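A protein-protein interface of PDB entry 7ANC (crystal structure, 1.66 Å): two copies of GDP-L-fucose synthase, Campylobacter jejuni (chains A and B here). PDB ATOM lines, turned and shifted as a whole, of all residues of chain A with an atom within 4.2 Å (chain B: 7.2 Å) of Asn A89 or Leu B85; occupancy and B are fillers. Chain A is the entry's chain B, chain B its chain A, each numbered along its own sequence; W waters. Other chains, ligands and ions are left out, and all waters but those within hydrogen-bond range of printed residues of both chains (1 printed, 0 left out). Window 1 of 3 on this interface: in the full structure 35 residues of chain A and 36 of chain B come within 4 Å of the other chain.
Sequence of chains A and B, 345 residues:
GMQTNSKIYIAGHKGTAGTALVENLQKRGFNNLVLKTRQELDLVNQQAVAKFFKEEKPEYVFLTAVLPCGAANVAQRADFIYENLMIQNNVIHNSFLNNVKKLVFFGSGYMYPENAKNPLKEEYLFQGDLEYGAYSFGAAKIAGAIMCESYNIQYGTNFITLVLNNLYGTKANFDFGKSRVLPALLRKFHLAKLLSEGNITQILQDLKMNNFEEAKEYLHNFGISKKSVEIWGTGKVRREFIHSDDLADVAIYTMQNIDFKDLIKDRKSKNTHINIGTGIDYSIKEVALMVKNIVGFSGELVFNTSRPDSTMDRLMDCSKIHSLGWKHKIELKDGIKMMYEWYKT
The side-chain amide nitrogen (ND2) of Asn A89 sits at hydrogen-bond distance from the side-chain sulfur (SD) of Met B86. The side-chain sulfur of Met A86 sits at hydrogen-bond distance from the side-chain amide nitrogen of Asn B89 (3.6 Å).
O of Leu B85 lies close to OD1 of Asn B89 (3.3 Å). The backbone carbonyl oxygen (O) of Met B86 lies close to the side-chain amide nitrogen (ND2) of Asn B90 (3.3 Å). OD1 of Asn B89 sits close to SD of Met B147 (3.4 Å). The backbone carbonyl oxygen (O) of Leu A85 lies close to the side-chain amide oxygen (OD1) of Asn A89 (3.3 Å). The backbone carbonyl oxygen (O) of Met A86 sits close to the side-chain amide nitrogen (ND2) of Asn A90 (3.3 Å). The side-chain sulfur (SD) of Met A147 sits close to the side-chain amide oxygen (OD1) of Asn A89, 3.5 Å away.
Leu A85 touches Asn B89 (CB to ND2, 3.6 Å). Met A86 touches Met B86 (CE to CE, 3.8 Å). Tyr B82 touches Asn A89 (CE1 to O, 3.9 Å). ND2 of Asn A89 touches CB of Leu B85, at 3.5 Å. Asn B89 touches Asn A89 (ND2 to ND2, 3.7 Å). His A93 touches Tyr B82 (CD2 to OH, 3.4 Å). Ile B81 touches Met A147. Tyr B82 touches Met A147.
Of the printed residues of chain B, Met A86 touches Met B86 and Asn B89. Asn A89 touches just these residues of chain B: Tyr B82, Leu B85, Met B86 and Asn B89. Asn A90 touches none of the printed residues of chain B. Printed residues of chain A within 4 Å of Tyr B82: Asn A89, His A93 and Met A147. Glu B83 touches none of the printed residues of chain A. Of chain A, only Asn A89 (3.5 Å) comes within 4 Å of Leu B85. Printed residues of chain A within 4 Å of Met B86: Met A86 (3.8 Å) and Asn A89 (3.6 Å). Printed residues of chain A within 4 Å of Asn B89: Leu A85, Met A86 and Asn A89.
Hydrophobic or aromatic side chains of chain B that line the printed part of chain A: Ile B81, Tyr B82, Leu B85 and Met B86. Of the 10 printed residues of chain A, 5 touch a printed residue of chain B. Hydrophobic or aromatic side chains of chain A that line the printed part of chain B: Leu A85, Met A86, His A93 and Met A147. Among the printed residues, 10 pairs touch across the chains. Among the printed residues, no Asp or Glu carboxylate lies within 4 Å of a Lys or Arg side-chain nitrogen of the other chain.
Leu A85 touches Asn B89, and with the chains exchanged Asn A89 touches Leu B85. Met A86 touches its own counterpart, Met B86. Met A86 touches Asn B89, and with the chains exchanged Asn A89 touches Met B86. Asn B89 touches its own counterpart, Asn A89. Positions printed for both chains: 85, 86, 87, 88, 89, 90, 91 and 147.
Water W1 lies within hydrogen-bond range of OD1 of Asn A90 (2.8 Å) and OH of Tyr B82 (2.9 Å).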
ATOM      1  N   LEU A  85      19.569   8.735 -29.968  1.00  0.00           N
ATOM      2  CA  LEU A  85      20.898   8.125 -29.904  1.00  0.00           C
ATOM      3  C   LEU A  85      21.107   7.077 -31.014  1.00  0.00           C
ATOM      4  O   LEU A  85      22.208   7.017 -31.589  1.00  0.00           O
ATOM      5  CB  LEU A  85      21.185   7.441 -28.536  1.00  0.00           C
ATOM      6  CG  LEU A  85      21.373   8.366 -27.345  1.00  0.00           C
ATOM      7  CD1 LEU A  85      21.548   7.534 -26.056  1.00  0.00           C
ATOM      8  CD2 LEU A  85      22.555   9.337 -27.510  1.00  0.00           C
ATOM      9  N   MET A  86      20.075   6.265 -31.334  1.00  0.00           N
ATOM     10  CA  MET A  86      20.260   5.239 -32.387  1.00  0.00           C
ATOM     11  C   MET A  86      20.457   5.881 -33.809  1.00  0.00           C
ATOM     12  O   MET A  86      21.349   5.479 -34.556  1.00  0.00           O
ATOM     13  CB  MET A  86      19.115   4.231 -32.401  1.00  0.00           C
ATOM     14  CG  MET A  86      19.038   3.289 -31.191  1.00  0.00           C
ATOM     15  SD  MET A  86      20.515   2.275 -30.954  1.00  0.00           S
ATOM     16  CE  MET A  86      20.571   1.403 -32.527  1.00  0.00           C
ATOM     17  N   ILE A  87      19.653   6.897 -34.122  1.00  0.00           N
ATOM     18  CA  ILE A  87      19.755   7.606 -35.425  1.00  0.00           C
ATOM     19  C   ILE A  87      21.192   8.207 -35.543  1.00  0.00           C
ATOM     20  O   ILE A  87      21.893   8.001 -36.561  1.00  0.00           O
ATOM     21  CB  ILE A  87      18.686   8.686 -35.532  1.00  0.00           C
ATOM     22  CG1 ILE A  87      17.293   8.053 -35.706  1.00  0.00           C
ATOM     23  CG2 ILE A  87      18.966   9.653 -36.699  1.00  0.00           C
ATOM     24  CD1 ILE A  87      16.158   9.053 -35.524  1.00  0.00           C
ATOM     25  N   GLN A  88      21.614   8.960 -34.504  1.00  0.00           N
ATOM     26  CA  GLN A  88      22.946   9.569 -34.441  1.00  0.00           C
ATOM     27  C   GLN A  88      24.078   8.548 -34.588  1.00  0.00           C
ATOM     28  O   GLN A  88      24.971   8.667 -35.476  1.00  0.00           O
ATOM     29  CB  GLN A  88      23.152  10.394 -33.150  1.00  0.00           C
ATOM     30  CG  GLN A  88      22.223  11.591 -33.020  1.00  0.00           C
ATOM     31  CD  GLN A  88      22.033  12.173 -31.589  1.00  0.00           C
ATOM     32  OE1 GLN A  88      21.149  13.005 -31.427  1.00  0.00           O
ATOM     33  NE2 GLN A  88      22.779  11.722 -30.592  1.00  0.00           N
ATOM     34  N   ASN A  89      24.026   7.496 -33.763  1.00  0.00           N
ATOM     35  CA  ASN A  89      25.046   6.474 -33.784  1.00  0.00           C
ATOM     36  C   ASN A  89      25.117   5.747 -35.148  1.00  0.00           C
ATOM     37  O   ASN A  89      26.230   5.526 -35.697  1.00  0.00           O
ATOM     38  CB  ASN A  89      24.844   5.450 -32.630  1.00  0.00           C
ATOM     39  CG  ASN A  89      25.039   6.042 -31.225  1.00  0.00           C
ATOM     40  OD1 ASN A  89      25.447   7.176 -31.033  1.00  0.00           O
ATOM     41  ND2 ASN A  89      24.720   5.214 -30.225  1.00  0.00           N
ATOM     42  N   ASN A  90      23.969   5.323 -35.668  1.00  0.00           N
ATOM     43  CA  ASN A  90      23.911   4.555 -36.918  1.00  0.00           C
ATOM     44  C   ASN A  90      24.473   5.385 -38.099  1.00  0.00           C
ATOM     45  O   ASN A  90      25.339   4.909 -38.882  1.00  0.00           O
ATOM     46  CB  ASN A  90      22.492   4.105 -37.219  1.00  0.00           C
ATOM     47  CG  ASN A  90      22.007   2.902 -36.329  1.00  0.00           C
ATOM     48  OD1 ASN A  90      22.795   2.177 -35.744  1.00  0.00           O
ATOM     49  ND2 ASN A  90      20.701   2.748 -36.231  1.00  0.00           N
ATOM     50  N   VAL A  91      24.042   6.650 -38.194  1.00  0.00           N
ATOM     51  CA  VAL A  91      24.431   7.502 -39.333  1.00  0.00           C
ATOM     52  C   VAL A  91      25.925   7.941 -39.200  1.00  0.00           C
ATOM     53  O   VAL A  91      26.700   7.858 -40.183  1.00  0.00           O
ATOM     54  CB  VAL A  91      23.496   8.696 -39.538  1.00  0.00           C
ATOM     55  CG1 VAL A  91      24.060   9.642 -40.582  1.00  0.00           C
ATOM     56  CG2 VAL A  91      22.124   8.224 -39.918  1.00  0.00           C
ATOM     57  N   ILE A  92      26.342   8.401 -38.010  1.00  0.00           N
ATOM     58  CA  ILE A  92      27.726   8.851 -37.795  1.00  0.00           C
ATOM     59  C   ILE A  92      28.748   7.711 -37.965  1.00  0.00           C
ATOM     60  O   ILE A  92      29.753   7.865 -38.693  1.00  0.00           O
ATOM     61  CB  ILE A  92      27.907   9.592 -36.448  1.00  0.00           C
ATOM     62  CG1 ILE A  92      27.106  10.913 -36.460  1.00  0.00           C
ATOM     63  CG2 ILE A  92      29.379   9.871 -36.172  1.00  0.00           C
ATOM     64  CD1 ILE A  92      26.893  11.527 -35.070  1.00  0.00           C
ATOM     65  N   HIS A  93      28.508   6.571 -37.294  1.00  0.00           N
ATOM     66  CA  HIS A  93      29.482   5.489 -37.339  1.00  0.00           C
ATOM     67  C   HIS A  93      29.565   4.897 -38.777  1.00  0.00           C
ATOM     68  O   HIS A  93      30.660   4.620 -39.251  1.00  0.00           O
ATOM     69  CB  HIS A  93      29.198   4.378 -36.308  1.00  0.00           C
ATOM     70  CG  HIS A  93      30.240   3.297 -36.293  1.00  0.00           C
ATOM     71  ND1 HIS A  93      31.515   3.511 -35.799  1.00  0.00           N
ATOM     72  CD2 HIS A  93      30.185   1.993 -36.687  1.00  0.00           C
ATOM     73  CE1 HIS A  93      32.209   2.381 -35.899  1.00  0.00           C
ATOM     74  NE2 HIS A  93      31.430   1.447 -36.438  1.00  0.00           N
ATOM     75  N   MET A 147      30.069  12.828 -29.882  1.00  0.00           N
ATOM     76  CA  MET A 147      30.378  11.797 -30.869  1.00  0.00           C
ATOM     77  C   MET A 147      31.113  12.397 -32.098  1.00  0.00           C
ATOM     78  O   MET A 147      32.203  11.921 -32.455  1.00  0.00           O
ATOM     79  CB  MET A 147      29.116  11.036 -31.266  1.00  0.00           C
ATOM     80  CG  MET A 147      29.295  10.125 -32.469  1.00  0.00           C
ATOM     81  SD  MET A 147      28.349   8.578 -32.324  1.00  0.00           S
ATOM     82  CE  MET A 147      29.339   8.144 -30.929  1.00  0.00           C
ATOM     83  N   ASP B  79      35.787   5.425 -29.881  1.00  0.00           N
ATOM     84  CA  ASP B  79      35.329   4.078 -29.509  1.00  0.00           C
ATOM     85  C   ASP B  79      34.635   4.069 -28.107  1.00  0.00           C
ATOM     86  O   ASP B  79      33.617   3.374 -27.901  1.00  0.00           O
ATOM     87  CB  ASP B  79      36.473   3.061 -29.524  1.00  0.00           C
ATOM     88  CG  ASP B  79      37.205   2.992 -30.885  1.00  0.00           C
ATOM     89  OD1 ASP B  79      36.615   3.346 -31.953  1.00  0.00           O
ATOM     90  OD2 ASP B  79      38.407   2.576 -30.857  1.00  0.00           O
ATOM     91  N   PHE B  80      35.189   4.829 -27.164  1.00  0.00           N
ATOM     92  CA  PHE B  80      34.623   4.858 -25.785  1.00  0.00           C
ATOM     93  C   PHE B  80      33.146   5.341 -25.785  1.00  0.00           C
ATOM     94  O   PHE B  80      32.338   4.850 -24.975  1.00  0.00           O
ATOM     95  CB  PHE B  80      35.354   5.777 -24.822  1.00  0.00           C
ATOM     96  CG  PHE B  80      36.779   5.388 -24.539  1.00  0.00           C
ATOM     97  CD1 PHE B  80      37.140   4.064 -24.310  1.00  0.00           C
ATOM     98  CD2 PHE B  80      37.770   6.362 -24.480  1.00  0.00           C
ATOM     99  CE1 PHE B  80      38.458   3.712 -24.066  1.00  0.00           C
ATOM    100  CE2 PHE B  80      39.088   6.020 -24.241  1.00  0.00           C
ATOM    101  CZ  PHE B  80      39.433   4.691 -24.028  1.00  0.00           C
ATOM    102  N   ILE B  81      32.819   6.330 -26.615  1.00  0.00           N
ATOM    103  CA  ILE B  81      31.418   6.787 -26.696  1.00  0.00           C
ATOM    104  C   ILE B  81      30.550   5.869 -27.583  1.00  0.00           C
ATOM    105  O   ILE B  81      29.486   5.419 -27.149  1.00  0.00           O
ATOM    106  CB  ILE B  81      31.303   8.325 -26.937  1.00  0.00           C
ATOM    107  CG1 ILE B  81      29.832   8.773 -26.939  1.00  0.00           C
ATOM    108  CG2 ILE B  81      32.017   8.772 -28.199  1.00  0.00           C
ATOM    109  CD1 ILE B  81      29.626  10.276 -26.765  1.00  0.00           C
ATOM    110  N   TYR B  82      30.983   5.563 -28.819  1.00  0.00           N
ATOM    111  CA  TYR B  82      30.175   4.742 -29.729  1.00  0.00           C
ATOM    112  C   TYR B  82      29.872   3.326 -29.170  1.00  0.00           C
ATOM    113  O   TYR B  82      28.707   2.896 -29.118  1.00  0.00           O
ATOM    114  CB  TYR B  82      30.798   4.634 -31.146  1.00  0.00           C
ATOM    115  CG  TYR B  82      30.052   3.678 -32.042  1.00  0.00           C
ATOM    116  CD1 TYR B  82      28.776   3.981 -32.531  1.00  0.00           C
ATOM    117  CD2 TYR B  82      30.548   2.391 -32.300  1.00  0.00           C
ATOM    118  CE1 TYR B  82      28.067   3.088 -33.328  1.00  0.00           C
ATOM    119  CE2 TYR B  82      29.844   1.478 -33.102  1.00  0.00           C
ATOM    120  CZ  TYR B  82      28.623   1.810 -33.608  1.00  0.00           C
ATOM    121  OH  TYR B  82      27.879   0.943 -34.398  1.00  0.00           O
ATOM    122  N   GLU B  83      30.916   2.599 -28.771  1.00  0.00           N
ATOM    123  CA  GLU B  83      30.726   1.211 -28.315  1.00  0.00           C
ATOM    124  C   GLU B  83      29.883   1.101 -27.047  1.00  0.00           C
ATOM    125  O   GLU B  83      28.953   0.284 -26.974  1.00  0.00           O
ATOM    126  CB  GLU B  83      32.068   0.464 -28.208  1.00  0.00           C
ATOM    127  CG  GLU B  83      32.744   0.367 -29.573  1.00  0.00           C
ATOM    128  CD  GLU B  83      34.004  -0.496 -29.591  1.00  0.00           C
ATOM    129  OE1 GLU B  83      34.174  -1.367 -28.684  1.00  0.00           O
ATOM    130  OE2 GLU B  83      34.833  -0.277 -30.517  1.00  0.00           O
ATOM    131  N   ASN B  84      30.168   1.952 -26.060  1.00  0.00           N
ATOM    132  CA  ASN B  84      29.418   1.951 -24.819  1.00  0.00           C
ATOM    133  C   ASN B  84      27.975   2.414 -25.002  1.00  0.00           C
ATOM    134  O   ASN B  84      27.033   1.793 -24.457  1.00  0.00           O
ATOM    135  CB  ASN B  84      30.164   2.715 -23.713  1.00  0.00           C
ATOM    136  CG  ASN B  84      31.410   1.980 -23.262  1.00  0.00           C
ATOM    137  OD1 ASN B  84      31.332   0.791 -22.909  1.00  0.00           O
ATOM    138  ND2 ASN B  84      32.571   2.652 -23.294  1.00  0.00           N
ATOM    139  N   LEU B  85      27.732   3.425 -25.842  1.00  0.00           N
ATOM    140  CA  LEU B  85      26.328   3.771 -26.132  1.00  0.00           C
ATOM    141  C   LEU B  85      25.587   2.616 -26.818  1.00  0.00           C
ATOM    142  O   LEU B  85      24.410   2.381 -26.515  1.00  0.00           O
ATOM    143  CB  LEU B  85      26.168   5.052 -26.989  1.00  0.00           C
ATOM    144  CG  LEU B  85      26.580   6.383 -26.348  1.00  0.00           C
ATOM    145  CD1 LEU B  85      26.477   7.478 -27.430  1.00  0.00           C
ATOM    146  CD2 LEU B  85      25.702   6.693 -25.154  1.00  0.00           C
ATOM    147  N   MET B  86      26.224   1.930 -27.788  1.00  0.00           N
ATOM    148  CA  MET B  86      25.540   0.822 -28.472  1.00  0.00           C
ATOM    149  C   MET B  86      25.215  -0.372 -27.533  1.00  0.00           C
ATOM    150  O   MET B  86      24.094  -0.897 -27.571  1.00  0.00           O
ATOM    151  CB  MET B  86      26.330   0.365 -29.713  1.00  0.00           C
ATOM    152  CG  MET B  86      26.351   1.326 -30.902  1.00  0.00           C
ATOM    153  SD  MET B  86      24.754   1.828 -31.555  1.00  0.00           S
ATOM    154  CE  MET B  86      24.119   0.207 -32.006  1.00  0.00           C
ATOM    155  N   ILE B  87      26.164  -0.758 -26.681  1.00  0.00           N
ATOM    156  CA  ILE B  87      25.984  -1.851 -25.700  1.00  0.00           C
ATOM    157  C   ILE B  87      24.784  -1.494 -24.785  1.00  0.00           C
ATOM    158  O   ILE B  87      23.825  -2.298 -24.593  1.00  0.00           O
ATOM    159  CB  ILE B  87      27.267  -2.079 -24.878  1.00  0.00           C
ATOM    160  CG1 ILE B  87      28.359  -2.661 -25.756  1.00  0.00           C
ATOM    161  CG2 ILE B  87      27.030  -2.985 -23.660  1.00  0.00           C
ATOM    162  CD1 ILE B  87      29.720  -2.675 -25.111  1.00  0.00           C
ATOM    163  N   GLN B  88      24.831  -0.288 -24.196  1.00  0.00           N
ATOM    164  CA  GLN B  88      23.733   0.221 -23.339  1.00  0.00           C
ATOM    165  C   GLN B  88      22.384   0.232 -24.052  1.00  0.00           C
ATOM    166  O   GLN B  88      21.383  -0.301 -23.549  1.00  0.00           O
ATOM    167  CB  GLN B  88      24.092   1.646 -22.807  1.00  0.00           C
ATOM    168  CG  GLN B  88      25.329   1.703 -21.916  1.00  0.00           C
ATOM    169  CD  GLN B  88      25.998   3.072 -21.707  1.00  0.00           C
ATOM    170  OE1 GLN B  88      27.068   3.115 -21.151  1.00  0.00           O
ATOM    171  NE2 GLN B  88      25.376   4.169 -22.181  1.00  0.00           N
ATOM    172  N   ASN B  89      22.325   0.867 -25.229  1.00  0.00           N
ATOM    173  CA  ASN B  89      21.096   0.950 -25.995  1.00  0.00           C
ATOM    174  C   ASN B  89      20.513  -0.424 -26.347  1.00  0.00           C
ATOM    175  O   ASN B  89      19.286  -0.675 -26.191  1.00  0.00           O
ATOM    176  CB  ASN B  89      21.268   1.784 -27.290  1.00  0.00           C
ATOM    177  CG  ASN B  89      21.580   3.275 -27.037  1.00  0.00           C
ATOM    178  OD1 ASN B  89      21.474   3.770 -25.934  1.00  0.00           O
ATOM    179  ND2 ASN B  89      21.933   3.981 -28.129  1.00  0.00           N
ATOM    180  N   ASN B  90      21.370  -1.289 -26.886  1.00  0.00           N
ATOM    181  CA  ASN B  90      20.913  -2.608 -27.366  1.00  0.00           C
ATOM    182  C   ASN B  90      20.350  -3.452 -26.195  1.00  0.00           C
ATOM    183  O   ASN B  90      19.235  -4.035 -26.290  1.00  0.00           O
ATOM    184  CB  ASN B  90      22.044  -3.325 -28.065  1.00  0.00           C
ATOM    185  CG  ASN B  90      22.357  -2.798 -29.481  1.00  0.00           C
ATOM    186  OD1 ASN B  90      21.546  -2.152 -30.127  1.00  0.00           O
ATOM    187  ND2 ASN B  90      23.557  -3.094 -29.947  1.00  0.00           N
ATOM    188  N   VAL B  91      21.081  -3.463 -25.075  1.00  0.00           N
ATOM    189  CA  VAL B  91      20.680  -4.289 -23.929  1.00  0.00           C
ATOM    190  C   VAL B  91      19.448  -3.722 -23.204  1.00  0.00           C
ATOM    191  O   VAL B  91      18.494  -4.471 -22.901  1.00  0.00           O
ATOM    192  CB  VAL B  91      21.841  -4.603 -22.971  1.00  0.00           C
ATOM    193  CG1 VAL B  91      21.331  -5.328 -21.740  1.00  0.00           C
ATOM    194  CG2 VAL B  91      22.903  -5.436 -23.677  1.00  0.00           C
ATOM    195  N   SER B 136      34.678  11.516 -23.106  1.00  0.00           N
ATOM    196  CA  SER B 136      33.714  10.822 -23.978  1.00  0.00           C
ATOM    197  C   SER B 136      33.129   9.565 -23.287  1.00  0.00           C
ATOM    198  O   SER B 136      31.936   9.251 -23.452  1.00  0.00           O
ATOM    199  CB  SER B 136      34.332  10.534 -25.351  1.00  0.00           C
ATOM    200  OG  SER B 136      35.340   9.563 -25.246  1.00  0.00           O
ATOM    201  N   ALA B 139      30.549  10.855 -20.700  1.00  0.00           N
ATOM    202  CA  ALA B 139      29.342  11.232 -21.398  1.00  0.00           C
ATOM    203  C   ALA B 139      28.484  10.009 -21.756  1.00  0.00           C
ATOM    204  O   ALA B 139      27.257  10.049 -21.597  1.00  0.00           O
ATOM    205  CB  ALA B 139      29.646  12.068 -22.650  1.00  0.00           C
ATOM    206  N   ALA B 140      29.124   8.918 -22.185  1.00  0.00           N
ATOM    207  CA  ALA B 140      28.379   7.660 -22.452  1.00  0.00           C
ATOM    208  C   ALA B 140      27.717   7.108 -21.197  1.00  0.00           C
ATOM    209  O   ALA B 140      26.545   6.715 -21.235  1.00  0.00           O
ATOM    210  CB  ALA B 140      29.284   6.625 -23.083  1.00  0.00           C
ATOM    211  N   LYS B 141      28.446   7.150 -20.076  1.00  0.00           N
ATOM    212  CA  LYS B 141      27.905   6.694 -18.784  1.00  0.00           C
ATOM    213  C   LYS B 141      26.738   7.541 -18.277  1.00  0.00           C
ATOM    214  O   LYS B 141      25.755   6.989 -17.762  1.00  0.00           O
ATOM    215  CB  LYS B 141      28.995   6.534 -17.713  1.00  0.00           C
ATOM    216  CG  LYS B 141      29.982   5.404 -18.003  1.00  0.00           C
ATOM    217  CD  LYS B 141      29.320   4.026 -18.045  1.00  0.00           C
ATOM    218  CE  LYS B 141      30.328   2.925 -17.791  1.00  0.00           C
ATOM    219  NZ  LYS B 141      29.682   1.568 -17.690  1.00  0.00           N
ATOM    220  N   ILE B 142      26.810   8.869 -18.474  1.00  0.00           N
ATOM    221  CA  ILE B 142      25.642   9.736 -18.180  1.00  0.00           C
ATOM    222  C   ILE B 142      24.427   9.304 -18.985  1.00  0.00           C
ATOM    223  O   ILE B 142      23.295   9.183 -18.451  1.00  0.00           O
ATOM    224  CB  ILE B 142      25.965  11.227 -18.476  1.00  0.00           C
ATOM    225  CG1 ILE B 142      27.004  11.759 -17.484  1.00  0.00           C
ATOM    226  CG2 ILE B 142      24.702  12.100 -18.511  1.00  0.00           C
ATOM    227  CD1 ILE B 142      27.518  13.139 -17.785  1.00  0.00           C
ATOM    228  N   ALA B 143      24.622   9.076 -20.291  1.00  0.00           N
ATOM    229  CA  ALA B 143      23.525   8.673 -21.170  1.00  0.00           C
ATOM    230  C   ALA B 143      22.903   7.334 -20.751  1.00  0.00           C
ATOM    231  O   ALA B 143      21.677   7.173 -20.818  1.00  0.00           O
ATOM    232  CB  ALA B 143      23.956   8.639 -22.635  1.00  0.00           C
ATOM    233  N   GLY B 144      23.743   6.396 -20.286  1.00  0.00           N
ATOM    234  CA  GLY B 144      23.260   5.134 -19.739  1.00  0.00           C
ATOM    235  C   GLY B 144      22.366   5.298 -18.486  1.00  0.00           C
ATOM    236  O   GLY B 144      21.292   4.692 -18.380  1.00  0.00           O
ATOM    237  N   MET B 147      19.092   6.962 -19.648  1.00  0.00           N
ATOM    238  CA  MET B 147      18.313   5.948 -20.320  1.00  0.00           C
ATOM    239  C   MET B 147      17.504   5.066 -19.318  1.00  0.00           C
ATOM    240  O   MET B 147      16.272   4.922 -19.442  1.00  0.00           O
ATOM    241  CB  MET B 147      19.196   5.095 -21.243  1.00  0.00           C
ATOM    242  CG  MET B 147      18.499   3.887 -21.810  1.00  0.00           C
ATOM    243  SD  MET B 147      19.087   3.517 -23.500  1.00  0.00           S
ATOM    244  CE  MET B 147      18.277   5.023 -24.024  1.00  0.00           C
HETATM  245  O   HOH W   1      25.539   1.494 -36.064  1.00  0.00           O
